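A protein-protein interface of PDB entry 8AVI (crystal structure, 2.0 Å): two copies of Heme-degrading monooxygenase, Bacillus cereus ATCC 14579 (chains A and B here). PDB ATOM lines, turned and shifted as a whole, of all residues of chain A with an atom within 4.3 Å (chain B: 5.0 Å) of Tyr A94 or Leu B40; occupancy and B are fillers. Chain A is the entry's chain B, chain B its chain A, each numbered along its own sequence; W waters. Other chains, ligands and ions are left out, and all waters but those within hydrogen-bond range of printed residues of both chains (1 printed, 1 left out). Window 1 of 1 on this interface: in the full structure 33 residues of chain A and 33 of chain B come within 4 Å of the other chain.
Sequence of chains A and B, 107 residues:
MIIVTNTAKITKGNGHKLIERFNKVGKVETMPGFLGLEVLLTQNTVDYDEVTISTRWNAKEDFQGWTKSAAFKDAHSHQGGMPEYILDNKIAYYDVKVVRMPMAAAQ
The backbone NH of Leu B41 is in hydrogen-bond range of the backbone carbonyl oxygen of Asp A95 (2.9 Å).
N of Gln B43 lies within hydrogen-bond range of O of Tyr A93 (2.8 Å).
The side-chain amide nitrogen of Gln B43 lies within hydrogen-bond range of the side-chain carboxylate of Asp A95 (3.1 Å).
The backbone carbonyl oxygen of Thr B52 is in hydrogen-bond range of the backbone NH of Leu B40 (2.8 Å).
OG1 of Thr B42 sits at hydrogen-bond distance from OE1 of Glu B50 (2.8 Å).
O of Ile A3 is in hydrogen-bond range of N of Tyr A94, at 2.8 Å.
Ile A3 touches Glu B38 (CD1 to OE2, 3.7 Å).
Tyr A93 touches Thr B42.
Leu B40 touches Tyr A94 (CB to CB, 3.9 Å).
Tyr A94 touches Leu B41.
Tyr A94 touches Thr B42 (CE1 to OG1, 3.3 Å).
O of Val B39 touches O of Asp A95, 3.9997 Å away.
Asp A95 touches Leu B40.
C of Val A96 touches O of Val B39, 3.8 Å away.
Val A96 touches Leu B40.
Ile A2 touches none of the printed residues of chain B.
Printed residues of chain B within 4 Å of Ile A3: Glu B38 (3.7 Å).
Tyr A94 touches just these residues of chain B: Leu B40, Leu B41 and Thr B42.
Of the printed residues of chain B, Val A96 touches Val B39 (3.8 Å) and Leu B40 (3.8 Å).
Printed residues of chain A within 4 Å of Glu B38: Ile A3 (3.7 Å).
Of the printed residues of chain A, Leu B40 touches Tyr A94, Asp A95 and Val A96.
Of the printed residues of chain A, Leu B41 touches Tyr A94 (3.6 Å) and Asp A95 (2.9 Å).
Glu B50 touches none of the printed residues of chain A.
Printed residues of chain B that touch a printed residue of chain A: Glu B38, Val B39, Leu B40, Leu B41, Thr B42 and Gln B43.
Hydrophobic or aromatic side chains of chain B that line the printed part of chain A: Leu B40.
Of the 8 printed residues of chain A, 5 touch a printed residue of chain B.
Hydrophobic or aromatic side chains of chain A within 4 Å of the printed part of chain B: Ile A3, Tyr A93, Tyr A94 and Val A96.
Among the printed residues, 12 pairs touch across the chains.
No position is printed for both chains.
Of the 12 pairs that touch across the chains among the printed residues, none has its exchanged pair printed and touching as well.
Water W1 bridges N of Tyr A93 (2.9 Å) and O of Gln B43 (2.9 Å).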
ATOM      1  N   ILE A   2     -34.958 -14.193 -11.957  1.00  0.00           N
ATOM      2  CA  ILE A   2     -33.965 -13.484 -11.163  1.00  0.00           C
ATOM      3  C   ILE A   2     -33.159 -14.470 -10.337  1.00  0.00           C
ATOM      4  O   ILE A   2     -33.591 -15.595 -10.075  1.00  0.00           O
ATOM      5  CB  ILE A   2     -34.576 -12.442 -10.208  1.00  0.00           C
ATOM      6  CG1 ILE A   2     -35.386 -13.146  -9.121  1.00  0.00           C
ATOM      7  CG2 ILE A   2     -35.431 -11.424 -10.961  1.00  0.00           C
ATOM      8  CD1 ILE A   2     -35.710 -12.232  -7.938  1.00  0.00           C
ATOM      9  N   ILE A   3     -31.989 -14.007  -9.894  1.00  0.00           N
ATOM     10  CA  ILE A   3     -31.134 -14.763  -8.988  1.00  0.00           C
ATOM     11  C   ILE A   3     -30.815 -13.896  -7.781  1.00  0.00           C
ATOM     12  O   ILE A   3     -30.531 -12.702  -7.922  1.00  0.00           O
ATOM     13  CB  ILE A   3     -29.848 -15.232  -9.705  1.00  0.00           C
ATOM     14  CG1 ILE A   3     -30.203 -16.210 -10.821  1.00  0.00           C
ATOM     15  CG2 ILE A   3     -28.887 -15.874  -8.712  1.00  0.00           C
ATOM     16  CD1 ILE A   3     -29.002 -16.687 -11.620  1.00  0.00           C
ATOM     17  N   THR A   5     -28.345 -13.943  -4.362  1.00  0.00           N
ATOM     18  CA  THR A   5     -27.124 -14.575  -3.891  1.00  0.00           C
ATOM     19  C   THR A   5     -26.716 -13.974  -2.551  1.00  0.00           C
ATOM     20  O   THR A   5     -26.643 -12.750  -2.409  1.00  0.00           O
ATOM     21  CB  THR A   5     -26.014 -14.381  -4.928  1.00  0.00           C
ATOM     22  OG1 THR A   5     -26.138 -15.364  -5.966  1.00  0.00           O
ATOM     23  CG2 THR A   5     -24.671 -14.471  -4.300  1.00  0.00           C
ATOM     24  N   ALA A  92     -26.818  -9.984  -3.099  1.00  0.00           N
ATOM     25  CA  ALA A  92     -26.911  -9.371  -4.425  1.00  0.00           C
ATOM     26  C   ALA A  92     -28.117  -9.932  -5.175  1.00  0.00           C
ATOM     27  O   ALA A  92     -28.562 -11.049  -4.911  1.00  0.00           O
ATOM     28  CB  ALA A  92     -25.614  -9.590  -5.225  1.00  0.00           C
ATOM     29  N   TYR A  93     -28.668  -9.133  -6.088  1.00  0.00           N
ATOM     30  CA  TYR A  93     -29.796  -9.519  -6.930  1.00  0.00           C
ATOM     31  C   TYR A  93     -29.405  -9.375  -8.395  1.00  0.00           C
ATOM     32  O   TYR A  93     -28.772  -8.390  -8.781  1.00  0.00           O
ATOM     33  CB  TYR A  93     -31.037  -8.641  -6.661  1.00  0.00           C
ATOM     34  CG  TYR A  93     -31.424  -8.569  -5.224  1.00  0.00           C
ATOM     35  CD1 TYR A  93     -30.809  -7.677  -4.364  1.00  0.00           C
ATOM     36  CD2 TYR A  93     -32.403  -9.413  -4.711  1.00  0.00           C
ATOM     37  CE1 TYR A  93     -31.155  -7.624  -3.020  1.00  0.00           C
ATOM     38  CE2 TYR A  93     -32.760  -9.365  -3.367  1.00  0.00           C
ATOM     39  CZ  TYR A  93     -32.125  -8.472  -2.532  1.00  0.00           C
ATOM     40  OH  TYR A  93     -32.467  -8.416  -1.209  1.00  0.00           O
ATOM     41  N   TYR A  94     -29.809 -10.342  -9.216  1.00  0.00           N
ATOM     42  CA  TYR A  94     -29.464 -10.343 -10.622  1.00  0.00           C
ATOM     43  C   TYR A  94     -30.716 -10.589 -11.443  1.00  0.00           C
ATOM     44  O   TYR A  94     -31.580 -11.387 -11.060  1.00  0.00           O
ATOM     45  CB  TYR A  94     -28.407 -11.429 -10.944  1.00  0.00           C
ATOM     46  CG  TYR A  94     -27.140 -11.348 -10.116  1.00  0.00           C
ATOM     47  CD1 TYR A  94     -26.045 -10.601 -10.553  1.00  0.00           C
ATOM     48  CD2 TYR A  94     -27.021 -12.054  -8.911  1.00  0.00           C
ATOM     49  CE1 TYR A  94     -24.867 -10.541  -9.814  1.00  0.00           C
ATOM     50  CE2 TYR A  94     -25.855 -11.987  -8.157  1.00  0.00           C
ATOM     51  CZ  TYR A  94     -24.778 -11.223  -8.621  1.00  0.00           C
ATOM     52  OH  TYR A  94     -23.625 -11.160  -7.884  1.00  0.00           O
ATOM     53  N   ASP A  95     -30.811  -9.889 -12.562  1.00  0.00           N
ATOM     54  CA  ASP A  95     -31.786 -10.192 -13.595  1.00  0.00           C
ATOM     55  C   ASP A  95     -31.104 -11.049 -14.654  1.00  0.00           C
ATOM     56  O   ASP A  95     -30.021 -10.696 -15.131  1.00  0.00           O
ATOM     57  CB  ASP A  95     -32.326  -8.907 -14.224  1.00  0.00           C
ATOM     58  CG  ASP A  95     -33.225  -8.135 -13.274  1.00  0.00           C
ATOM     59  OD1 ASP A  95     -34.127  -8.757 -12.671  1.00  0.00           O
ATOM     60  OD2 ASP A  95     -33.022  -6.918 -13.113  1.00  0.00           O
ATOM     61  N   VAL A  96     -31.753 -12.147 -15.026  1.00  0.00           N
ATOM     62  CA  VAL A  96     -31.251 -13.023 -16.076  1.00  0.00           C
ATOM     63  C   VAL A  96     -31.643 -12.458 -17.433  1.00  0.00           C
ATOM     64  O   VAL A  96     -32.833 -12.363 -17.759  1.00  0.00           O
ATOM     65  CB  VAL A  96     -31.777 -14.452 -15.886  1.00  0.00           C
ATOM     66  CG1 VAL A  96     -31.206 -15.360 -16.949  1.00  0.00           C
ATOM     67  CG2 VAL A  96     -31.386 -14.961 -14.471  1.00  0.00           C
ATOM     68  N   GLU B  38     -25.277 -18.236 -18.900  1.00  0.00           N
ATOM     69  CA  GLU B  38     -26.257 -17.179 -18.632  1.00  0.00           C
ATOM     70  C   GLU B  38     -25.543 -15.846 -18.490  1.00  0.00           C
ATOM     71  O   GLU B  38     -24.378 -15.784 -18.080  1.00  0.00           O
ATOM     72  CB  GLU B  38     -27.113 -17.454 -17.361  1.00  0.00           C
ATOM     73  CG  GLU B  38     -26.299 -17.717 -16.109  1.00  0.00           C
ATOM     74  CD  GLU B  38     -27.132 -18.192 -14.907  1.00  0.00           C
ATOM     75  OE1 GLU B  38     -28.357 -18.419 -15.062  1.00  0.00           O
ATOM     76  OE2 GLU B  38     -26.537 -18.341 -13.807  1.00  0.00           O
ATOM     77  N   VAL B  39     -26.254 -14.780 -18.855  1.00  0.00           N
ATOM     78  CA  VAL B  39     -25.782 -13.410 -18.724  1.00  0.00           C
ATOM     79  C   VAL B  39     -26.686 -12.695 -17.728  1.00  0.00           C
ATOM     80  O   VAL B  39     -27.913 -12.680 -17.891  1.00  0.00           O
ATOM     81  CB  VAL B  39     -25.778 -12.689 -20.091  1.00  0.00           C
ATOM     82  CG1 VAL B  39     -25.217 -11.286 -19.938  1.00  0.00           C
ATOM     83  CG2 VAL B  39     -24.970 -13.466 -21.137  1.00  0.00           C
ATOM     84  N   LEU B  40     -26.085 -12.092 -16.709  1.00  0.00           N
ATOM     85  CA  LEU B  40     -26.818 -11.462 -15.624  1.00  0.00           C
ATOM     86  C   LEU B  40     -26.499  -9.982 -15.580  1.00  0.00           C
ATOM     87  O   LEU B  40     -25.351  -9.574 -15.792  1.00  0.00           O
ATOM     88  CB  LEU B  40     -26.446 -12.053 -14.268  1.00  0.00           C
ATOM     89  CG  LEU B  40     -26.330 -13.578 -14.259  1.00  0.00           C
ATOM     90  CD1 LEU B  40     -25.749 -14.029 -12.918  1.00  0.00           C
ATOM     91  CD2 LEU B  40     -27.718 -14.129 -14.428  1.00  0.00           C
ATOM     92  N   LEU B  41     -27.500  -9.193 -15.208  1.00  0.00           N
ATOM     93  CA  LEU B  41     -27.320  -7.767 -14.944  1.00  0.00           C
ATOM     94  C   LEU B  41     -27.620  -7.521 -13.476  1.00  0.00           C
ATOM     95  O   LEU B  41     -28.731  -7.810 -13.016  1.00  0.00           O
ATOM     96  CB  LEU B  41     -28.244  -6.908 -15.814  1.00  0.00           C
ATOM     97  CG  LEU B  41     -28.011  -5.408 -15.559  1.00  0.00           C
ATOM     98  CD1 LEU B  41     -26.677  -5.024 -16.117  1.00  0.00           C
ATOM     99  CD2 LEU B  41     -29.111  -4.549 -16.152  1.00  0.00           C
ATOM    100  N   THR B  42     -26.628  -7.021 -12.745  1.00  0.00           N
ATOM    101  CA  THR B  42     -26.761  -6.799 -11.312  1.00  0.00           C
ATOM    102  C   THR B  42     -27.791  -5.710 -11.027  1.00  0.00           C
ATOM    103  O   THR B  42     -27.877  -4.722 -11.753  1.00  0.00           O
ATOM    104  CB  THR B  42     -25.400  -6.410 -10.726  1.00  0.00           C
ATOM    105  OG1 THR B  42     -24.466  -7.467 -10.961  1.00  0.00           O
ATOM    106  CG2 THR B  42     -25.488  -6.151  -9.220  1.00  0.00           C
ATOM    107  N   GLN B  43     -28.592  -5.899  -9.977  1.00  0.00           N
ATOM    108  CA  GLN B  43     -29.565  -4.883  -9.588  1.00  0.00           C
ATOM    109  C   GLN B  43     -28.926  -3.854  -8.664  1.00  0.00           C
ATOM    110  O   GLN B  43     -27.989  -4.153  -7.918  1.00  0.00           O
ATOM    111  CB  GLN B  43     -30.783  -5.503  -8.906  1.00  0.00           C
ATOM    112  CG  GLN B  43     -31.800  -6.058  -9.882  1.00  0.00           C
ATOM    113  CD  GLN B  43     -33.036  -6.605  -9.190  1.00  0.00           C
ATOM    114  OE1 GLN B  43     -33.266  -6.356  -8.001  1.00  0.00           O
ATOM    115  NE2 GLN B  43     -33.835  -7.367  -9.933  1.00  0.00           N
ATOM    116  N   GLU B  50     -23.049  -3.660 -13.892  1.00  0.00           N
ATOM    117  CA  GLU B  50     -22.313  -4.902 -13.672  1.00  0.00           C
ATOM    118  C   GLU B  50     -22.992  -6.026 -14.442  1.00  0.00           C
ATOM    119  O   GLU B  50     -24.155  -6.356 -14.177  1.00  0.00           O
ATOM    120  CB  GLU B  50     -22.218  -5.241 -12.178  1.00  0.00           C
ATOM    121  CG  GLU B  50     -21.149  -6.284 -11.833  1.00  0.00           C
ATOM    122  CD  GLU B  50     -21.049  -6.548 -10.331  1.00  0.00           C
ATOM    123  OE1 GLU B  50     -21.984  -7.156  -9.766  1.00  0.00           O
ATOM    124  OE2 GLU B  50     -20.046  -6.140  -9.709  1.00  0.00           O
ATOM    125  N   VAL B  51     -22.264  -6.605 -15.390  1.00  0.00           N
ATOM    126  CA  VAL B  51     -22.756  -7.680 -16.244  1.00  0.00           C
ATOM    127  C   VAL B  51     -21.899  -8.906 -15.982  1.00  0.00           C
ATOM    128  O   VAL B  51     -20.667  -8.822 -16.022  1.00  0.00           O
ATOM    129  CB  VAL B  51     -22.699  -7.289 -17.732  1.00  0.00           C
ATOM    130  CG1 VAL B  51     -23.011  -8.489 -18.624  1.00  0.00           C
ATOM    131  CG2 VAL B  51     -23.666  -6.119 -18.025  1.00  0.00           C
ATOM    132  N   THR B  52     -22.544 -10.039 -15.704  1.00  0.00           N
ATOM    133  CA  THR B  52     -21.854 -11.292 -15.404  1.00  0.00           C
ATOM    134  C   THR B  52     -22.155 -12.302 -16.502  1.00  0.00           C
ATOM    135  O   THR B  52     -23.324 -12.556 -16.814  1.00  0.00           O
ATOM    136  CB  THR B  52     -22.280 -11.828 -14.030  1.00  0.00           C
ATOM    137  OG1 THR B  52     -22.015 -10.843 -13.023  1.00  0.00           O
ATOM    138  CG2 THR B  52     -21.528 -13.119 -13.666  1.00  0.00           C
HETATM  139  O   HOH W   1     -27.686  -6.406  -6.066  1.00  0.00           O
